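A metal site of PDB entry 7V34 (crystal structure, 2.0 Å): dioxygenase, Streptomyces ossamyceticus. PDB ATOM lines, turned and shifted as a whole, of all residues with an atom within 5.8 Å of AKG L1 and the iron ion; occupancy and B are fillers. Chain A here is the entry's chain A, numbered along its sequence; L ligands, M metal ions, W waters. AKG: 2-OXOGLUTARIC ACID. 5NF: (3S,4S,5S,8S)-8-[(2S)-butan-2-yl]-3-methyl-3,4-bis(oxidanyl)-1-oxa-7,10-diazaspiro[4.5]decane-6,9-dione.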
ATOM      1  N   LEU A 118      -6.389  -4.046 -11.746  1.00  0.00           N
ATOM      2  CA  LEU A 118      -7.550  -3.842 -10.875  1.00  0.00           C
ATOM      3  C   LEU A 118      -7.480  -2.553 -10.065  1.00  0.00           C
ATOM      4  O   LEU A 118      -6.458  -2.214  -9.471  1.00  0.00           O
ATOM      5  CB  LEU A 118      -7.633  -5.025  -9.922  1.00  0.00           C
ATOM      6  CG  LEU A 118      -8.725  -5.056  -8.858  1.00  0.00           C
ATOM      7  CD1 LEU A 118     -10.071  -5.161  -9.554  1.00  0.00           C
ATOM      8  CD2 LEU A 118      -8.480  -6.255  -7.982  1.00  0.00           C
ATOM      9  N   GLN A 120     -10.341  -1.037  -6.974  1.00  0.00           N
ATOM     10  CA  GLN A 120     -11.461  -1.577  -6.195  1.00  0.00           C
ATOM     11  C   GLN A 120     -12.125  -0.516  -5.332  1.00  0.00           C
ATOM     12  O   GLN A 120     -11.504   0.477  -4.944  1.00  0.00           O
ATOM     13  CB  GLN A 120     -10.998  -2.703  -5.245  1.00  0.00           C
ATOM     14  CG  GLN A 120     -10.535  -3.918  -5.957  1.00  0.00           C
ATOM     15  CD  GLN A 120     -10.206  -5.027  -4.995  1.00  0.00           C
ATOM     16  OE1 GLN A 120      -9.271  -4.903  -4.207  1.00  0.00           O
ATOM     17  NE2 GLN A 120     -10.988  -6.111  -5.032  1.00  0.00           N
ATOM     18  N   THR A 182     -17.616  -5.671  -2.522  1.00  0.00           N
ATOM     19  CA  THR A 182     -16.415  -5.116  -3.122  1.00  0.00           C
ATOM     20  C   THR A 182     -16.594  -5.058  -4.632  1.00  0.00           C
ATOM     21  O   THR A 182     -16.968  -6.063  -5.244  1.00  0.00           O
ATOM     22  CB  THR A 182     -15.195  -5.968  -2.774  1.00  0.00           C
ATOM     23  OG1 THR A 182     -14.939  -5.843  -1.371  1.00  0.00           O
ATOM     24  CG2 THR A 182     -13.941  -5.552  -3.575  1.00  0.00           C
ATOM     25  N   ASN A 184     -15.067  -4.146  -8.487  1.00  0.00           N
ATOM     26  CA  ASN A 184     -13.806  -4.306  -9.205  1.00  0.00           C
ATOM     27  C   ASN A 184     -13.910  -3.708 -10.604  1.00  0.00           C
ATOM     28  O   ASN A 184     -14.890  -3.949 -11.306  1.00  0.00           O
ATOM     29  CB  ASN A 184     -13.445  -5.790  -9.367  1.00  0.00           C
ATOM     30  CG  ASN A 184     -13.228  -6.489  -8.050  1.00  0.00           C
ATOM     31  OD1 ASN A 184     -12.796  -5.895  -7.071  1.00  0.00           O
ATOM     32  ND2 ASN A 184     -13.515  -7.770  -8.028  1.00  0.00           N
ATOM     33  N   TYR A 186     -11.211  -3.360 -14.035  1.00  0.00           N
ATOM     34  CA  TYR A 186      -9.908  -3.654 -14.621  1.00  0.00           C
ATOM     35  C   TYR A 186      -9.551  -2.585 -15.646  1.00  0.00           C
ATOM     36  O   TYR A 186     -10.278  -2.384 -16.618  1.00  0.00           O
ATOM     37  CB  TYR A 186      -9.924  -5.075 -15.208  1.00  0.00           C
ATOM     38  CG  TYR A 186     -10.195  -6.070 -14.089  1.00  0.00           C
ATOM     39  CD1 TYR A 186      -9.139  -6.625 -13.370  1.00  0.00           C
ATOM     40  CD2 TYR A 186     -11.508  -6.364 -13.673  1.00  0.00           C
ATOM     41  CE1 TYR A 186      -9.361  -7.513 -12.296  1.00  0.00           C
ATOM     42  CE2 TYR A 186     -11.748  -7.242 -12.590  1.00  0.00           C
ATOM     43  CZ  TYR A 186     -10.670  -7.818 -11.911  1.00  0.00           C
ATOM     44  OH  TYR A 186     -10.878  -8.667 -10.833  1.00  0.00           O
ATOM     45  N   LEU A 195      -5.602  -9.399 -12.365  1.00  0.00           N
ATOM     46  CA  LEU A 195      -5.480  -9.542 -10.919  1.00  0.00           C
ATOM     47  C   LEU A 195      -4.606 -10.764 -10.683  1.00  0.00           C
ATOM     48  O   LEU A 195      -4.888 -11.829 -11.234  1.00  0.00           O
ATOM     49  CB  LEU A 195      -6.853  -9.691 -10.230  1.00  0.00           C
ATOM     50  CG  LEU A 195      -6.896 -10.185  -8.781  1.00  0.00           C
ATOM     51  CD1 LEU A 195      -6.086  -9.281  -7.844  1.00  0.00           C
ATOM     52  CD2 LEU A 195      -8.347 -10.289  -8.286  1.00  0.00           C
ATOM     53  N   HIS A 198      -4.177 -15.707  -6.702  1.00  0.00           N
ATOM     54  CA  HIS A 198      -4.384 -15.552  -5.271  1.00  0.00           C
ATOM     55  C   HIS A 198      -5.486 -16.496  -4.804  1.00  0.00           C
ATOM     56  O   HIS A 198      -6.262 -17.044  -5.592  1.00  0.00           O
ATOM     57  CB  HIS A 198      -4.763 -14.109  -4.913  1.00  0.00           C
ATOM     58  CG  HIS A 198      -6.126 -13.737  -5.381  1.00  0.00           C
ATOM     59  ND1 HIS A 198      -6.420 -13.508  -6.711  1.00  0.00           N
ATOM     60  CD2 HIS A 198      -7.295 -13.620  -4.711  1.00  0.00           C
ATOM     61  CE1 HIS A 198      -7.701 -13.243  -6.841  1.00  0.00           C
ATOM     62  NE2 HIS A 198      -8.257 -13.303  -5.639  1.00  0.00           N
ATOM     63  N   LYS A 199      -5.559 -16.644  -3.494  1.00  0.00           N
ATOM     64  CA  LYS A 199      -6.696 -17.210  -2.789  1.00  0.00           C
ATOM     65  C   LYS A 199      -7.370 -16.092  -2.022  1.00  0.00           C
ATOM     66  O   LYS A 199      -6.700 -15.187  -1.508  1.00  0.00           O
ATOM     67  CB  LYS A 199      -6.231 -18.315  -1.827  1.00  0.00           C
ATOM     68  CG  LYS A 199      -5.601 -19.532  -2.547  1.00  0.00           C
ATOM     69  CD  LYS A 199      -4.878 -20.450  -1.557  1.00  0.00           C
ATOM     70  CE  LYS A 199      -4.599 -21.829  -2.137  1.00  0.00           C
ATOM     71  NZ  LYS A 199      -4.150 -22.778  -1.080  1.00  0.00           N
ATOM     72  N   ASP A 200      -8.707 -16.122  -1.964  1.00  0.00           N
ATOM     73  CA  ASP A 200      -9.428 -15.163  -1.136  1.00  0.00           C
ATOM     74  C   ASP A 200      -9.181 -15.443   0.336  1.00  0.00           C
ATOM     75  O   ASP A 200      -8.771 -16.545   0.720  1.00  0.00           O
ATOM     76  CB  ASP A 200     -10.924 -15.200  -1.444  1.00  0.00           C
ATOM     77  CG  ASP A 200     -11.233 -14.707  -2.839  1.00  0.00           C
ATOM     78  OD1 ASP A 200     -10.325 -14.068  -3.402  1.00  0.00           O
ATOM     79  OD2 ASP A 200     -12.333 -14.929  -3.377  1.00  0.00           O
ATOM     80  N   THR A 205     -16.788 -16.614  -1.028  1.00  0.00           N
ATOM     81  CA  THR A 205     -16.927 -15.473  -1.922  1.00  0.00           C
ATOM     82  C   THR A 205     -18.061 -15.766  -2.883  1.00  0.00           C
ATOM     83  O   THR A 205     -18.083 -16.822  -3.525  1.00  0.00           O
ATOM     84  CB  THR A 205     -15.634 -15.230  -2.717  1.00  0.00           C
ATOM     85  OG1 THR A 205     -14.555 -15.000  -1.817  1.00  0.00           O
ATOM     86  CG2 THR A 205     -15.788 -14.023  -3.656  1.00  0.00           C
ATOM     87  N   LEU A 207     -19.223 -14.326  -6.242  1.00  0.00           N
ATOM     88  CA  LEU A 207     -18.680 -13.445  -7.262  1.00  0.00           C
ATOM     89  C   LEU A 207     -19.685 -13.265  -8.388  1.00  0.00           C
ATOM     90  O   LEU A 207     -20.168 -14.251  -8.956  1.00  0.00           O
ATOM     91  CB  LEU A 207     -17.361 -14.000  -7.803  1.00  0.00           C
ATOM     92  CG  LEU A 207     -16.692 -13.113  -8.853  1.00  0.00           C
ATOM     93  CD1 LEU A 207     -16.168 -11.814  -8.200  1.00  0.00           C
ATOM     94  CD2 LEU A 207     -15.565 -13.881  -9.541  1.00  0.00           C
ATOM     95  N   THR A 209     -19.779 -12.033 -12.010  1.00  0.00           N
ATOM     96  CA  THR A 209     -18.972 -11.710 -13.177  1.00  0.00           C
ATOM     97  C   THR A 209     -19.779 -11.970 -14.443  1.00  0.00           C
ATOM     98  O   THR A 209     -20.518 -12.954 -14.526  1.00  0.00           O
ATOM     99  CB  THR A 209     -17.659 -12.535 -13.181  1.00  0.00           C
ATOM    100  OG1 THR A 209     -16.845 -12.095 -14.265  1.00  0.00           O
ATOM    101  CG2 THR A 209     -17.933 -14.030 -13.332  1.00  0.00           C
ATOM    102  N   LEU A 214     -11.696 -14.350 -15.697  1.00  0.00           N
ATOM    103  CA  LEU A 214     -11.440 -15.173 -14.531  1.00  0.00           C
ATOM    104  C   LEU A 214     -10.891 -16.542 -14.939  1.00  0.00           C
ATOM    105  O   LEU A 214     -11.455 -17.223 -15.796  1.00  0.00           O
ATOM    106  CB  LEU A 214     -12.729 -15.337 -13.717  1.00  0.00           C
ATOM    107  CG  LEU A 214     -12.615 -16.101 -12.394  1.00  0.00           C
ATOM    108  CD1 LEU A 214     -11.668 -15.387 -11.375  1.00  0.00           C
ATOM    109  CD2 LEU A 214     -14.015 -16.289 -11.813  1.00  0.00           C
ATOM    110  N   ASN A 235     -16.664 -19.429  -4.536  1.00  0.00           N
ATOM    111  CA  ASN A 235     -15.482 -20.175  -4.159  1.00  0.00           C
ATOM    112  C   ASN A 235     -15.199 -19.992  -2.689  1.00  0.00           C
ATOM    113  O   ASN A 235     -15.780 -19.130  -2.011  1.00  0.00           O
ATOM    114  CB  ASN A 235     -14.272 -19.807  -5.009  1.00  0.00           C
ATOM    115  CG  ASN A 235     -13.953 -18.336  -4.979  1.00  0.00           C
ATOM    116  OD1 ASN A 235     -13.448 -17.830  -3.983  1.00  0.00           O
ATOM    117  ND2 ASN A 235     -14.199 -17.660  -6.099  1.00  0.00           N
ATOM    118  N   HIS A 256      -6.932 -18.488  -8.014  1.00  0.00           N
ATOM    119  CA  HIS A 256      -7.535 -17.911  -9.211  1.00  0.00           C
ATOM    120  C   HIS A 256      -6.911 -16.546  -9.531  1.00  0.00           C
ATOM    121  O   HIS A 256      -6.196 -15.945  -8.732  1.00  0.00           O
ATOM    122  CB  HIS A 256      -9.050 -17.810  -9.063  1.00  0.00           C
ATOM    123  CG  HIS A 256      -9.497 -17.031  -7.869  1.00  0.00           C
ATOM    124  ND1 HIS A 256      -9.370 -17.507  -6.577  1.00  0.00           N
ATOM    125  CD2 HIS A 256     -10.043 -15.803  -7.757  1.00  0.00           C
ATOM    126  CE1 HIS A 256      -9.816 -16.604  -5.724  1.00  0.00           C
ATOM    127  NE2 HIS A 256     -10.237 -15.557  -6.427  1.00  0.00           N
ATOM    128  N   VAL A 258      -7.184 -13.059 -12.709  1.00  0.00           N
ATOM    129  CA  VAL A 258      -7.843 -12.440 -13.856  1.00  0.00           C
ATOM    130  C   VAL A 258      -6.763 -12.104 -14.870  1.00  0.00           C
ATOM    131  O   VAL A 258      -5.816 -11.380 -14.565  1.00  0.00           O
ATOM    132  CB  VAL A 258      -8.632 -11.175 -13.466  1.00  0.00           C
ATOM    133  CG1 VAL A 258      -9.247 -10.545 -14.719  1.00  0.00           C
ATOM    134  CG2 VAL A 258      -9.744 -11.505 -12.423  1.00  0.00           C
ATOM    135  N   ARG A 265     -13.016  -4.285 -17.951  1.00  0.00           N
ATOM    136  CA  ARG A 265     -13.812  -5.346 -17.352  1.00  0.00           C
ATOM    137  C   ARG A 265     -14.232  -4.882 -15.966  1.00  0.00           C
ATOM    138  O   ARG A 265     -13.503  -4.137 -15.302  1.00  0.00           O
ATOM    139  CB  ARG A 265     -13.007  -6.654 -17.291  1.00  0.00           C
ATOM    140  CG  ARG A 265     -13.768  -7.897 -16.768  1.00  0.00           C
ATOM    141  CD  ARG A 265     -12.793  -9.095 -16.663  1.00  0.00           C
ATOM    142  NE  ARG A 265     -13.406 -10.316 -16.147  1.00  0.00           N
ATOM    143  CZ  ARG A 265     -13.527 -10.589 -14.843  1.00  0.00           C
ATOM    144  NH1 ARG A 265     -13.096  -9.728 -13.938  1.00  0.00           N
ATOM    145  NH2 ARG A 265     -14.085 -11.730 -14.455  1.00  0.00           N
ATOM    146  N   SER A 266     -15.417  -5.290 -15.532  1.00  0.00           N
ATOM    147  CA  SER A 266     -15.825  -5.040 -14.156  1.00  0.00           C
ATOM    148  C   SER A 266     -16.532  -6.274 -13.608  1.00  0.00           C
ATOM    149  O   SER A 266     -16.937  -7.166 -14.352  1.00  0.00           O
ATOM    150  CB  SER A 266     -16.711  -3.779 -14.026  1.00  0.00           C
ATOM    151  OG  SER A 266     -17.958  -3.968 -14.683  1.00  0.00           O
ATOM    152  N   SER A 267     -16.675  -6.293 -12.280  1.00  0.00           N
ATOM    153  CA  SER A 267     -17.273  -7.400 -11.539  1.00  0.00           C
ATOM    154  C   SER A 267     -17.455  -6.922 -10.104  1.00  0.00           C
ATOM    155  O   SER A 267     -16.956  -5.860  -9.708  1.00  0.00           O
ATOM    156  CB  SER A 267     -16.395  -8.654 -11.599  1.00  0.00           C
ATOM    157  OG  SER A 267     -15.179  -8.438 -10.901  1.00  0.00           O
ATOM    158  N   PHE A 271     -17.952 -10.972   0.085  1.00  0.00           N
ATOM    159  CA  PHE A 271     -16.926 -11.733   0.771  1.00  0.00           C
ATOM    160  C   PHE A 271     -17.328 -11.901   2.236  1.00  0.00           C
ATOM    161  O   PHE A 271     -17.678 -10.912   2.893  1.00  0.00           O
ATOM    162  CB  PHE A 271     -15.564 -11.025   0.703  1.00  0.00           C
ATOM    163  CG  PHE A 271     -14.997 -10.916  -0.705  1.00  0.00           C
ATOM    164  CD1 PHE A 271     -15.483  -9.966  -1.594  1.00  0.00           C
ATOM    165  CD2 PHE A 271     -13.955 -11.753  -1.114  1.00  0.00           C
ATOM    166  CE1 PHE A 271     -14.941  -9.857  -2.893  1.00  0.00           C
ATOM    167  CE2 PHE A 271     -13.400 -11.643  -2.392  1.00  0.00           C
ATOM    168  CZ  PHE A 271     -13.906 -10.705  -3.283  1.00  0.00           C
HETATM  169  C1  AKG L   1     -11.388 -10.869  -6.134  1.00  0.00           C
HETATM  170  O1  AKG L   1     -10.826 -11.420  -5.159  1.00  0.00           O
HETATM  171  O2  AKG L   1     -11.881  -9.741  -5.997  1.00  0.00           O
HETATM  172  C2  AKG L   1     -11.460 -11.524  -7.434  1.00  0.00           C
HETATM  173  O5  AKG L   1     -10.975 -12.629  -7.609  1.00  0.00           O
HETATM  174  C3  AKG L   1     -12.159 -10.839  -8.597  1.00  0.00           C
HETATM  175  C4  AKG L   1     -12.327 -11.883  -9.712  1.00  0.00           C
HETATM  176  C5  AKG L   1     -13.033 -11.262 -10.912  1.00  0.00           C
HETATM  177  O3  AKG L   1     -13.627 -12.005 -11.707  1.00  0.00           O
HETATM  178  O4  AKG L   1     -13.031 -10.012 -11.059  1.00  0.00           O
HETATM  179  C1  5NF L   2      -8.194  -8.601  -1.615  1.00  0.00           C
HETATM  180  C2  5NF L   2      -8.574  -9.069  -3.021  1.00  0.00           C
HETATM  181  C3  5NF L   2     -10.120  -9.496  -2.857  1.00  0.00           C
HETATM  182  C4  5NF L   2     -10.475  -9.166  -1.359  1.00  0.00           C
HETATM  183  C5  5NF L   2     -10.507 -10.345  -0.341  1.00  0.00           C
HETATM  184  C6  5NF L   2     -12.574  -8.385  -0.199  1.00  0.00           C
HETATM  185  C10 5NF L   2     -10.735  -7.571   2.047  1.00  0.00           C
HETATM  186  C11 5NF L   2     -10.526  -6.501   3.127  1.00  0.00           C
HETATM  187  C12 5NF L   2      -7.637 -10.189  -3.506  1.00  0.00           C
HETATM  188  C7  5NF L   2     -12.362  -9.288   1.047  1.00  0.00           C
HETATM  189  C8  5NF L   2     -11.985  -8.415   2.281  1.00  0.00           C
HETATM  190  C9  5NF L   2     -11.778  -9.327   3.526  1.00  0.00           C
HETATM  191  N1  5NF L   2     -11.674  -8.386  -1.240  1.00  0.00           N
HETATM  192  N2  5NF L   2     -11.389 -10.334   0.723  1.00  0.00           N
HETATM  193  O1  5NF L   2      -8.512  -8.007  -3.887  1.00  0.00           O
HETATM  194  O2  5NF L   2     -10.970  -8.727  -3.660  1.00  0.00           O
HETATM  195  O3  5NF L   2      -9.374  -8.375  -0.895  1.00  0.00           O
HETATM  196  O4  5NF L   2      -9.747 -11.311  -0.482  1.00  0.00           O
HETATM  197  O5  5NF L   2     -13.527  -7.635  -0.336  1.00  0.00           O
HETATM  198 FE    FE M   1     -10.483 -13.540  -5.548  1.00  0.00          FE
HETATM  199  O   HOH W   1     -12.826 -13.791  -5.718  1.00  0.00           O
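O2 of 5NF L2 lies within hydrogen-bond range of O2 of AKG L1.
NH2 of Arg 265 is in salt-bridge range of O3 of AKG L1, at 2.8 Å.
The side-chain amide nitrogen (NE2) of Gln 120 is in hydrogen-bond range of an oxygen (O2) of 5NF L2, at 3.0 Å.
O4 of AKG L1 lies within hydrogen-bond range of OH of Tyr 186, 2.5 Å away.
The side-chain hydroxyl (OG1) of Thr 182 lies within hydrogen-bond range of an oxygen (O5) of 5NF L2.
An oxygen (O4) of AKG L1 lies within hydrogen-bond range of the side-chain hydroxyl of Ser 267, at 2.7 Å.
The side-chain amide nitrogen (ND2) of Asn 184 is in hydrogen-bond range of an oxygen (O2) of AKG L1 (3.3 Å).
NE2 of Gln 120 touches O2 of AKG L1, at 3.9 Å.
Leu 195 touches AKG L1.
CD2 of Leu 207 touches O3 of AKG L1 (3.5 Å).
Leu 214 touches AKG L1.
Val 258 touches AKG L1 (CG2 to C5, 3.6 Å).
Phe 271 touches AKG L1 (CZ to O2, 3.5 Å).
Hydrophobic or aromatic side chains that line AKG L1: Tyr 186, Leu 195, His 198, Leu 207, Leu 214, His 256, Val 258 and Phe 271.
Of the 20 residues printed, 13 come within 4 Å of AKG L1.
The iron ion is bound by an oxygen (O1) of AKG L1 (2.2 Å), a ring nitrogen (NE2) of His 256 (2.2 Å), the side-chain carboxylate (OD1) of Asp 200 (2.2 Å), a ring nitrogen (NE2) of His 198 (2.2 Å), an oxygen (O5) of AKG L1 (2.3 Å) and water W1 (2.4 Å).
The iron ion has six donor atoms within binding distance.
OD2 of Asp 200 sits close to OD1 of Asn 235, at 3.2 Å.
The backbone NH (N) of Tyr 186 lies within hydrogen-bond range of the backbone carbonyl oxygen (O) of Arg 265, at 2.7 Å.
NH2 of Arg 265 lies within hydrogen-bond range of OG1 of Thr 209 (2.8 Å).
OD1 of Asn 184 lies within hydrogen-bond range of NE2 of Gln 120 (2.7 Å).
The backbone NH (N) of Leu 195 lies within hydrogen-bond range of the backbone carbonyl oxygen (O) of Val 258, at 3.0 Å.
OD2 of Asp 200 is in hydrogen-bond range of OG1 of Thr 205 (2.7 Å).
O of Ser 267 is in hydrogen-bond range of N of Asn 184 (2.8 Å).
Of the 20 residues printed, 3 come within 4 Å of the iron ion.
The nearest printed residue that does not touch the iron ion is Phe 271 (4.7 Å).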
